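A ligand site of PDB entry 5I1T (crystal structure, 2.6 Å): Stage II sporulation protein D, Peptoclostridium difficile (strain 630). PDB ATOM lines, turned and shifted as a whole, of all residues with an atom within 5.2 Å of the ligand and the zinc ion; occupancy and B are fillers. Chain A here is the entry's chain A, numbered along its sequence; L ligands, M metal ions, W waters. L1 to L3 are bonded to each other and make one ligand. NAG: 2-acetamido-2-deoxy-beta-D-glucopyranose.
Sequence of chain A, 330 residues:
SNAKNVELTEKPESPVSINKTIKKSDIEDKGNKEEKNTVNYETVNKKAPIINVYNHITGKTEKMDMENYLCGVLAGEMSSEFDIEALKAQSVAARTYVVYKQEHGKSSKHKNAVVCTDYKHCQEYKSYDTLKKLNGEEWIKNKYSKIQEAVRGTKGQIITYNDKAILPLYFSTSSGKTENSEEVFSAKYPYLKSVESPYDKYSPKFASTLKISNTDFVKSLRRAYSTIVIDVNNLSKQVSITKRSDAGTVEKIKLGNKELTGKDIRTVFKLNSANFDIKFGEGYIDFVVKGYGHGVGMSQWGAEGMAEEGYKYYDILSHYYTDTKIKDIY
Lys 120 touches the ligand.
Leu 167 touches the ligand.
CD2 of Leu 169 touches O3 of NAG L1 (3.2 Å).
CB of Phe 185 touches O7 of NAG L3, at 3.3 Å.
CE2 of Tyr 189 touches C8 of NAG L3, 3.3 Å away.
Hydrophobic or aromatic side chains that line the ligand: Tyr 97, His 121, Leu 167, Leu 169, Tyr 170, Phe 185, Ala 187, Tyr 189 and His 294.
Within 4 Å of the ligand: Tyr 97, Tyr 119, Lys 120, His 121, Cys 122, Leu 167, Leu 169, Tyr 170, Phe 185, Ser 186, Ala 187, Tyr 189 and His 294.
The nearest printed residue that does not touch the ligand is Pro 168 (4.1 Å).
Water W5 lies within hydrogen-bond range of an oxygen (O1) of NAG L1 (2.4 Å), the backbone carbonyl oxygen of Tyr 170 (2.5 Å) and a ring nitrogen (NE2) of His 294 (3.3 Å).
Water W4 lies within hydrogen-bond range of the backbone carbonyl oxygen of His 121 (2.8 Å) and an oxygen (O4) of NAG L1 (3.5 Å).
The zinc ion is bound by ND1 of His 121 (2.2 Å), NE2 of His 110 (2.2 Å), SG of Cys 122 (2.3 Å) and SG of Cys 116 (2.3 Å).
Within 4 Å of the zinc ion: His 110, Cys 116, His 121 and Cys 122.
The nearest printed residue that does not touch the zinc ion is Val 115 (4.3 Å).
A nitrogen (N2) of NAG L1 sits at hydrogen-bond distance from the backbone carbonyl oxygen (O) of Cys 122 (2.9 Å).
The backbone NH (N) of Ala 187 is in hydrogen-bond range of an oxygen (O7) of NAG L3 (2.6 Å).
A ring nitrogen (NE2) of His 294 sits at hydrogen-bond distance from an oxygen (O7) of NAG L1.
An oxygen (O7) of NAG L3 is in hydrogen-bond range of the backbone NH (N) of Ser 186, at 2.8 Å.
The backbone carbonyl oxygen (O) of Tyr 119 lies within hydrogen-bond range of an oxygen (O1) of NAG L1, 3.0 Å away.
An oxygen (O7) of NAG L1 lies within hydrogen-bond range of the backbone NH (N) of Tyr 170, 3.0 Å away.
The side-chain hydroxyl of Tyr 97 is in hydrogen-bond range of an oxygen (O3) of NAG L1 (3.2 Å).
The backbone carbonyl oxygen (O) of His 121 lies within hydrogen-bond range of the side-chain hydroxyl (OH) of Tyr 97 (3.4 Å).
O of Ala 187 sits at hydrogen-bond distance from OG of Ser 181 (2.7 Å).
A ring nitrogen (NE2) of His 294 is in hydrogen-bond range of the backbone carbonyl oxygen of Tyr 170.
The side-chain hydroxyl (OH) of Tyr 170 is in hydrogen-bond range of the side-chain amide oxygen (OE1) of Gln 123 (2.5 Å).
The side-chain carboxylate of Asp 118 lies close to the backbone NH of Lys 120 (3.0 Å).
The backbone NH (N) of Tyr 189 is in hydrogen-bond range of the side-chain hydroxyl (OG) of Ser 181 (3.3 Å).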
ATOM      1  N   TYR A  97      34.434  -8.503 -23.358  1.00  0.00           N
ATOM      2  CA  TYR A  97      34.123  -9.439 -22.264  1.00  0.00           C
ATOM      3  C   TYR A  97      35.118 -10.590 -22.293  1.00  0.00           C
ATOM      4  O   TYR A  97      35.703 -10.941 -21.278  1.00  0.00           O
ATOM      5  CB  TYR A  97      32.691  -9.965 -22.395  1.00  0.00           C
ATOM      6  CG  TYR A  97      32.120 -10.590 -21.145  1.00  0.00           C
ATOM      7  CD1 TYR A  97      32.350 -11.924 -20.847  1.00  0.00           C
ATOM      8  CD2 TYR A  97      31.339  -9.840 -20.267  1.00  0.00           C
ATOM      9  CE1 TYR A  97      31.824 -12.503 -19.696  1.00  0.00           C
ATOM     10  CE2 TYR A  97      30.811 -10.399 -19.104  1.00  0.00           C
ATOM     11  CZ  TYR A  97      31.043 -11.731 -18.829  1.00  0.00           C
ATOM     12  OH  TYR A  97      30.507 -12.311 -17.687  1.00  0.00           O
ATOM     13  N   LYS A 101      38.184 -11.358 -19.543  1.00  0.00           N
ATOM     14  CA  LYS A 101      38.310 -12.653 -18.865  1.00  0.00           C
ATOM     15  C   LYS A 101      39.667 -13.306 -19.091  1.00  0.00           C
ATOM     16  O   LYS A 101      40.204 -13.901 -18.181  1.00  0.00           O
ATOM     17  CB  LYS A 101      37.200 -13.618 -19.272  1.00  0.00           C
ATOM     18  CG  LYS A 101      35.789 -13.207 -18.879  1.00  0.00           C
ATOM     19  CD  LYS A 101      35.520 -13.284 -17.392  1.00  0.00           C
ATOM     20  CE  LYS A 101      34.066 -12.964 -17.135  1.00  0.00           C
ATOM     21  NZ  LYS A 101      33.701 -13.103 -15.698  1.00  0.00           N
ATOM     22  N   HIS A 110      33.913 -22.856 -15.049  1.00  0.00           N
ATOM     23  CA  HIS A 110      34.596 -23.458 -16.197  1.00  0.00           C
ATOM     24  C   HIS A 110      36.060 -23.001 -16.239  1.00  0.00           C
ATOM     25  O   HIS A 110      36.389 -22.025 -16.906  1.00  0.00           O
ATOM     26  CB  HIS A 110      33.846 -23.095 -17.499  1.00  0.00           C
ATOM     27  CG  HIS A 110      33.426 -21.655 -17.595  1.00  0.00           C
ATOM     28  ND1 HIS A 110      34.290 -20.633 -17.923  1.00  0.00           N
ATOM     29  CD2 HIS A 110      32.213 -21.067 -17.433  1.00  0.00           C
ATOM     30  CE1 HIS A 110      33.637 -19.487 -17.941  1.00  0.00           C
ATOM     31  NE2 HIS A 110      32.371 -19.726 -17.664  1.00  0.00           N
ATOM     32  N   VAL A 115      35.180 -18.057 -21.479  1.00  0.00           N
ATOM     33  CA  VAL A 115      33.765 -17.721 -21.385  1.00  0.00           C
ATOM     34  C   VAL A 115      32.930 -18.975 -21.647  1.00  0.00           C
ATOM     35  O   VAL A 115      33.455 -19.980 -22.141  1.00  0.00           O
ATOM     36  CB  VAL A 115      33.359 -16.649 -22.436  1.00  0.00           C
ATOM     37  CG1 VAL A 115      34.019 -15.313 -22.128  1.00  0.00           C
ATOM     38  CG2 VAL A 115      33.705 -17.120 -23.852  1.00  0.00           C
ATOM     39  N   CYS A 116      31.653 -18.909 -21.290  1.00  0.00           N
ATOM     40  CA  CYS A 116      30.749 -20.032 -21.546  1.00  0.00           C
ATOM     41  C   CYS A 116      29.524 -19.514 -22.283  1.00  0.00           C
ATOM     42  O   CYS A 116      29.291 -18.314 -22.331  1.00  0.00           O
ATOM     43  CB  CYS A 116      30.346 -20.764 -20.273  1.00  0.00           C
ATOM     44  SG  CYS A 116      29.318 -19.834 -19.117  1.00  0.00           S
ATOM     45  N   ASP A 118      26.369 -19.646 -21.529  1.00  0.00           N
ATOM     46  CA  ASP A 118      25.218 -19.414 -20.637  1.00  0.00           C
ATOM     47  C   ASP A 118      25.099 -17.926 -20.253  1.00  0.00           C
ATOM     48  O   ASP A 118      25.964 -17.365 -19.560  1.00  0.00           O
ATOM     49  CB  ASP A 118      25.354 -20.304 -19.395  1.00  0.00           C
ATOM     50  CG  ASP A 118      24.130 -20.266 -18.481  1.00  0.00           C
ATOM     51  OD1 ASP A 118      23.139 -19.560 -18.785  1.00  0.00           O
ATOM     52  OD2 ASP A 118      24.163 -20.958 -17.445  1.00  0.00           O
ATOM     53  N   TYR A 119      24.011 -17.280 -20.689  1.00  0.00           N
ATOM     54  CA  TYR A 119      23.773 -15.864 -20.404  1.00  0.00           C
ATOM     55  C   TYR A 119      23.650 -15.567 -18.896  1.00  0.00           C
ATOM     56  O   TYR A 119      23.757 -14.414 -18.490  1.00  0.00           O
ATOM     57  CB  TYR A 119      22.513 -15.362 -21.154  1.00  0.00           C
ATOM     58  CG  TYR A 119      21.170 -15.818 -20.588  1.00  0.00           C
ATOM     59  CD1 TYR A 119      20.612 -17.040 -20.934  1.00  0.00           C
ATOM     60  CD2 TYR A 119      20.450 -14.993 -19.715  1.00  0.00           C
ATOM     61  CE1 TYR A 119      19.398 -17.444 -20.411  1.00  0.00           C
ATOM     62  CE2 TYR A 119      19.223 -15.395 -19.188  1.00  0.00           C
ATOM     63  CZ  TYR A 119      18.705 -16.623 -19.545  1.00  0.00           C
ATOM     64  OH  TYR A 119      17.499 -17.036 -19.040  1.00  0.00           O
ATOM     65  N   LYS A 120      23.422 -16.605 -18.097  1.00  0.00           N
ATOM     66  CA  LYS A 120      23.319 -16.467 -16.626  1.00  0.00           C
ATOM     67  C   LYS A 120      24.698 -16.372 -15.958  1.00  0.00           C
ATOM     68  O   LYS A 120      24.798 -15.991 -14.785  1.00  0.00           O
ATOM     69  CB  LYS A 120      22.534 -17.629 -16.020  1.00  0.00           C
ATOM     70  CG  LYS A 120      21.085 -17.682 -16.476  1.00  0.00           C
ATOM     71  CD  LYS A 120      20.417 -18.984 -16.076  1.00  0.00           C
ATOM     72  CE  LYS A 120      19.034 -19.070 -16.680  1.00  0.00           C
ATOM     73  NZ  LYS A 120      18.432 -20.404 -16.428  1.00  0.00           N
ATOM     74  N   HIS A 121      25.746 -16.742 -16.698  1.00  0.00           N
ATOM     75  CA  HIS A 121      27.093 -16.679 -16.158  1.00  0.00           C
ATOM     76  C   HIS A 121      27.997 -15.691 -16.921  1.00  0.00           C
ATOM     77  O   HIS A 121      28.624 -14.827 -16.278  1.00  0.00           O
ATOM     78  CB  HIS A 121      27.745 -18.061 -16.110  1.00  0.00           C
ATOM     79  CG  HIS A 121      29.014 -18.062 -15.335  1.00  0.00           C
ATOM     80  ND1 HIS A 121      30.255 -17.975 -15.925  1.00  0.00           N
ATOM     81  CD2 HIS A 121      29.227 -18.039 -14.002  1.00  0.00           C
ATOM     82  CE1 HIS A 121      31.181 -17.960 -14.981  1.00  0.00           C
ATOM     83  NE2 HIS A 121      30.583 -17.983 -13.806  1.00  0.00           N
ATOM     84  N   CYS A 122      28.061 -15.836 -18.261  1.00  0.00           N
ATOM     85  CA  CYS A 122      28.870 -14.922 -19.116  1.00  0.00           C
ATOM     86  C   CYS A 122      27.958 -14.167 -20.072  1.00  0.00           C
ATOM     87  O   CYS A 122      27.510 -13.054 -19.753  1.00  0.00           O
ATOM     88  CB  CYS A 122      30.002 -15.656 -19.879  1.00  0.00           C
ATOM     89  SG  CYS A 122      31.377 -16.274 -18.867  1.00  0.00           S
ATOM     90  N   GLN A 123      27.697 -14.749 -21.245  1.00  0.00           N
ATOM     91  CA  GLN A 123      26.819 -14.119 -22.231  1.00  0.00           C
ATOM     92  C   GLN A 123      26.220 -15.179 -23.129  1.00  0.00           C
ATOM     93  O   GLN A 123      26.691 -16.317 -23.188  1.00  0.00           O
ATOM     94  CB  GLN A 123      27.540 -13.022 -23.012  1.00  0.00           C
ATOM     95  CG  GLN A 123      28.897 -13.396 -23.594  1.00  0.00           C
ATOM     96  CD  GLN A 123      29.658 -12.189 -24.147  1.00  0.00           C
ATOM     97  OE1 GLN A 123      29.189 -11.056 -24.080  1.00  0.00           O
ATOM     98  NE2 GLN A 123      30.846 -12.449 -24.701  1.00  0.00           N
ATOM     99  N   LEU A 167      35.491  -4.616 -17.663  1.00  0.00           N
ATOM    100  CA  LEU A 167      34.470  -5.644 -17.448  1.00  0.00           C
ATOM    101  C   LEU A 167      33.226  -4.994 -18.049  1.00  0.00           C
ATOM    102  O   LEU A 167      32.582  -4.201 -17.394  1.00  0.00           O
ATOM    103  CB  LEU A 167      34.258  -5.892 -15.962  1.00  0.00           C
ATOM    104  CG  LEU A 167      33.160  -6.909 -15.598  1.00  0.00           C
ATOM    105  CD1 LEU A 167      33.499  -8.320 -16.028  1.00  0.00           C
ATOM    106  CD2 LEU A 167      32.916  -6.855 -14.111  1.00  0.00           C
ATOM    107  N   PRO A 168      32.866  -5.337 -19.300  1.00  0.00           N
ATOM    108  CA  PRO A 168      31.800  -4.628 -19.984  1.00  0.00           C
ATOM    109  C   PRO A 168      30.425  -5.289 -19.784  1.00  0.00           C
ATOM    110  O   PRO A 168      29.893  -5.954 -20.694  1.00  0.00           O
ATOM    111  CB  PRO A 168      32.265  -4.764 -21.433  1.00  0.00           C
ATOM    112  CG  PRO A 168      32.854  -6.157 -21.471  1.00  0.00           C
ATOM    113  CD  PRO A 168      33.181  -6.555 -20.048  1.00  0.00           C
ATOM    114  N   LEU A 169      29.867  -5.115 -18.587  1.00  0.00           N
ATOM    115  CA  LEU A 169      28.582  -5.717 -18.278  1.00  0.00           C
ATOM    116  C   LEU A 169      27.493  -5.050 -19.109  1.00  0.00           C
ATOM    117  O   LEU A 169      27.585  -3.879 -19.469  1.00  0.00           O
ATOM    118  CB  LEU A 169      28.293  -5.628 -16.785  1.00  0.00           C
ATOM    119  CG  LEU A 169      29.368  -6.224 -15.830  1.00  0.00           C
ATOM    120  CD1 LEU A 169      28.970  -5.989 -14.373  1.00  0.00           C
ATOM    121  CD2 LEU A 169      29.637  -7.724 -16.063  1.00  0.00           C
ATOM    122  N   TYR A 170      26.483  -5.825 -19.463  1.00  0.00           N
ATOM    123  CA  TYR A 170      25.373  -5.290 -20.248  1.00  0.00           C
ATOM    124  C   TYR A 170      24.091  -6.098 -19.986  1.00  0.00           C
ATOM    125  O   TYR A 170      24.140  -7.252 -19.527  1.00  0.00           O
ATOM    126  CB  TYR A 170      25.740  -5.213 -21.755  1.00  0.00           C
ATOM    127  CG  TYR A 170      26.062  -6.524 -22.405  1.00  0.00           C
ATOM    128  CD1 TYR A 170      25.036  -7.381 -22.780  1.00  0.00           C
ATOM    129  CD2 TYR A 170      27.355  -6.885 -22.688  1.00  0.00           C
ATOM    130  CE1 TYR A 170      25.304  -8.598 -23.377  1.00  0.00           C
ATOM    131  CE2 TYR A 170      27.639  -8.108 -23.281  1.00  0.00           C
ATOM    132  CZ  TYR A 170      26.587  -8.952 -23.619  1.00  0.00           C
ATOM    133  OH  TYR A 170      26.823 -10.158 -24.205  1.00  0.00           O
ATOM    134  N   SER A 181      27.848  -0.550 -10.288  1.00  0.00           N
ATOM    135  CA  SER A 181      28.230  -1.953 -10.082  1.00  0.00           C
ATOM    136  C   SER A 181      28.102  -2.462  -8.643  1.00  0.00           C
ATOM    137  O   SER A 181      27.529  -3.527  -8.420  1.00  0.00           O
ATOM    138  CB  SER A 181      29.666  -2.166 -10.588  1.00  0.00           C
ATOM    139  OG  SER A 181      30.610  -1.243 -10.009  1.00  0.00           O
ATOM    140  N   PHE A 185      26.221  -5.717  -7.533  1.00  0.00           N
ATOM    141  CA  PHE A 185      27.124  -6.830  -7.266  1.00  0.00           C
ATOM    142  C   PHE A 185      27.963  -6.531  -6.029  1.00  0.00           C
ATOM    143  O   PHE A 185      27.383  -6.250  -4.965  1.00  0.00           O
ATOM    144  CB  PHE A 185      27.931  -7.219  -8.529  1.00  0.00           C
ATOM    145  CG  PHE A 185      27.065  -7.668  -9.682  1.00  0.00           C
ATOM    146  CD1 PHE A 185      26.375  -8.890  -9.618  1.00  0.00           C
ATOM    147  CD2 PHE A 185      26.942  -6.897 -10.843  1.00  0.00           C
ATOM    148  CE1 PHE A 185      25.575  -9.315 -10.678  1.00  0.00           C
ATOM    149  CE2 PHE A 185      26.165  -7.318 -11.905  1.00  0.00           C
ATOM    150  CZ  PHE A 185      25.478  -8.528 -11.834  1.00  0.00           C
ATOM    151  N   SER A 186      29.284  -6.559  -6.129  1.00  0.00           N
ATOM    152  CA  SER A 186      30.153  -6.354  -4.950  1.00  0.00           C
ATOM    153  C   SER A 186      31.102  -5.179  -5.045  1.00  0.00           C
ATOM    154  O   SER A 186      31.190  -4.392  -4.119  1.00  0.00           O
ATOM    155  CB  SER A 186      31.011  -7.592  -4.733  1.00  0.00           C
ATOM    156  OG  SER A 186      30.199  -8.726  -4.536  1.00  0.00           O
ATOM    157  N   ALA A 187      31.802  -5.064  -6.166  1.00  0.00           N
ATOM    158  CA  ALA A 187      32.819  -4.036  -6.346  1.00  0.00           C
ATOM    159  C   ALA A 187      32.432  -2.805  -7.160  1.00  0.00           C
ATOM    160  O   ALA A 187      31.547  -2.826  -8.034  1.00  0.00           O
ATOM    161  CB  ALA A 187      34.059  -4.677  -6.950  1.00  0.00           C
ATOM    162  N   TYR A 189      33.594   0.124  -9.790  1.00  0.00           N
ATOM    163  CA  TYR A 189      34.497   0.342 -10.951  1.00  0.00           C
ATOM    164  C   TYR A 189      34.241   1.729 -11.529  1.00  0.00           C
ATOM    165  O   TYR A 189      33.083   2.074 -11.771  1.00  0.00           O
ATOM    166  CB  TYR A 189      34.295  -0.698 -12.056  1.00  0.00           C
ATOM    167  CG  TYR A 189      34.822  -2.063 -11.717  1.00  0.00           C
ATOM    168  CD1 TYR A 189      36.181  -2.350 -11.796  1.00  0.00           C
ATOM    169  CD2 TYR A 189      33.961  -3.080 -11.352  1.00  0.00           C
ATOM    170  CE1 TYR A 189      36.670  -3.608 -11.483  1.00  0.00           C
ATOM    171  CE2 TYR A 189      34.439  -4.335 -11.058  1.00  0.00           C
ATOM    172  CZ  TYR A 189      35.775  -4.610 -11.115  1.00  0.00           C
ATOM    173  OH  TYR A 189      36.184  -5.872 -10.799  1.00  0.00           O
ATOM    174  N   LEU A 192      31.687   1.659 -14.420  1.00  0.00           N
ATOM    175  CA  LEU A 192      30.350   1.082 -14.261  1.00  0.00           C
ATOM    176  C   LEU A 192      29.556   1.972 -13.313  1.00  0.00           C
ATOM    177  O   LEU A 192      29.206   1.565 -12.228  1.00  0.00           O
ATOM    178  CB  LEU A 192      30.393  -0.364 -13.756  1.00  0.00           C
ATOM    179  CG  LEU A 192      31.157  -1.328 -14.670  1.00  0.00           C
ATOM    180  CD1 LEU A 192      31.159  -2.753 -14.134  1.00  0.00           C
ATOM    181  CD2 LEU A 192      30.555  -1.298 -16.072  1.00  0.00           C
ATOM    182  N   HIS A 294      20.216  -7.172 -15.044  1.00  0.00           N
ATOM    183  CA  HIS A 294      20.907  -6.682 -13.845  1.00  0.00           C
ATOM    184  C   HIS A 294      21.070  -5.169 -13.712  1.00  0.00           C
ATOM    185  O   HIS A 294      21.293  -4.664 -12.610  1.00  0.00           O
ATOM    186  CB  HIS A 294      22.218  -7.434 -13.594  1.00  0.00           C
ATOM    187  CG  HIS A 294      23.190  -7.354 -14.729  1.00  0.00           C
ATOM    188  ND1 HIS A 294      23.742  -6.167 -15.147  1.00  0.00           N
ATOM    189  CD2 HIS A 294      23.739  -8.308 -15.514  1.00  0.00           C
ATOM    190  CE1 HIS A 294      24.565  -6.394 -16.159  1.00  0.00           C
ATOM    191  NE2 HIS A 294      24.580  -7.689 -16.402  1.00  0.00           N
HETATM  192  C1  NAG L   1      25.222 -11.999 -17.080  1.00  0.00           C
HETATM  193  C2  NAG L   1      26.360 -11.005 -16.906  1.00  0.00           C
HETATM  194  C3  NAG L   1      27.389 -11.617 -15.974  1.00  0.00           C
HETATM  195  C4  NAG L   1      26.722 -11.974 -14.636  1.00  0.00           C
HETATM  196  C5  NAG L   1      25.449 -12.811 -14.869  1.00  0.00           C
HETATM  197  C6  NAG L   1      24.666 -13.063 -13.577  1.00  0.00           C
HETATM  198  C7  NAG L   1      27.056  -9.437 -18.664  1.00  0.00           C
HETATM  199  C8  NAG L   1      27.566  -9.331 -20.066  1.00  0.00           C
HETATM  200  N2  NAG L   1      26.936 -10.685 -18.202  1.00  0.00           N
HETATM  201  O1  NAG L   1      24.282 -11.510 -18.029  1.00  0.00           O
HETATM  202  O3  NAG L   1      28.456 -10.684 -15.786  1.00  0.00           O
HETATM  203  O4  NAG L   1      27.629 -12.714 -13.787  1.00  0.00           O
HETATM  204  O5  NAG L   1      24.597 -12.177 -15.812  1.00  0.00           O
HETATM  205  O6  NAG L   1      24.310 -11.824 -12.960  1.00  0.00           O
HETATM  206  O7  NAG L   1      26.743  -8.432 -18.013  1.00  0.00           O
HETATM  207  C1  NAG L   2      27.874 -12.046 -12.551  1.00  0.00           C
HETATM  208  C2  NAG L   2      28.437 -13.020 -11.521  1.00  0.00           C
HETATM  209  C3  NAG L   2      28.949 -12.285 -10.288  1.00  0.00           C
HETATM  210  C4  NAG L   2      29.861 -11.134 -10.669  1.00  0.00           C
HETATM  211  C5  NAG L   2      29.229 -10.234 -11.727  1.00  0.00           C
HETATM  212  C6  NAG L   2      30.200  -9.199 -12.266  1.00  0.00           C
HETATM  213  C7  NAG L   2      27.490 -15.290 -11.298  1.00  0.00           C
HETATM  214  C8  NAG L   2      26.308 -16.098 -10.834  1.00  0.00           C
HETATM  215  N2  NAG L   2      27.401 -13.974 -11.122  1.00  0.00           N
HETATM  216  O3  NAG L   2      29.673 -13.185  -9.459  1.00  0.00           O
HETATM  217  O4  NAG L   2      30.136 -10.370  -9.478  1.00  0.00           O
HETATM  218  O5  NAG L   2      28.805 -11.007 -12.835  1.00  0.00           O
HETATM  219  O6  NAG L   2      31.290  -9.850 -12.928  1.00  0.00           O
HETATM  220  O7  NAG L   2      28.457 -15.833 -11.817  1.00  0.00           O
HETATM  221  C1  NAG L   3      31.423 -10.622  -8.895  1.00  0.00           C
HETATM  222  C2  NAG L   3      31.956  -9.330  -8.272  1.00  0.00           C
HETATM  223  C3  NAG L   3      33.296  -9.561  -7.582  1.00  0.00           C
HETATM  224  C4  NAG L   3      33.229 -10.778  -6.648  1.00  0.00           C
HETATM  225  C5  NAG L   3      32.584 -11.987  -7.342  1.00  0.00           C
HETATM  226  C6  NAG L   3      32.409 -13.182  -6.408  1.00  0.00           C
HETATM  227  C7  NAG L   3      31.685  -7.098  -9.220  1.00  0.00           C
HETATM  228  C8  NAG L   3      31.789  -6.254 -10.454  1.00  0.00           C
HETATM  229  N2  NAG L   3      32.103  -8.350  -9.332  1.00  0.00           N
HETATM  230  O3  NAG L   3      33.680  -8.402  -6.842  1.00  0.00           O
HETATM  231  O4  NAG L   3      34.567 -11.091  -6.248  1.00  0.00           O
HETATM  232  O5  NAG L   3      31.312 -11.613  -7.883  1.00  0.00           O
HETATM  233  O6  NAG L   3      31.060 -13.254  -5.951  1.00  0.00           O
HETATM  234  O7  NAG L   3      31.208  -6.628  -8.199  1.00  0.00           O
HETATM  235 ZN    ZN M   1      30.712 -18.330 -17.996  1.00  0.00          ZN
HETATM  236  O   HOH W   1      23.960 -11.505 -20.722  1.00  0.00           O
HETATM  237  O   HOH W   2      24.882 -12.984  -9.802  1.00  0.00           O
HETATM  238  O   HOH W   3      33.692  -9.676 -11.427  1.00  0.00           O
HETATM  239  O   HOH W   4      30.583 -14.451 -14.308  1.00  0.00           O
HETATM  240  O   HOH W   5      23.235  -9.484 -18.790  1.00  0.00           O
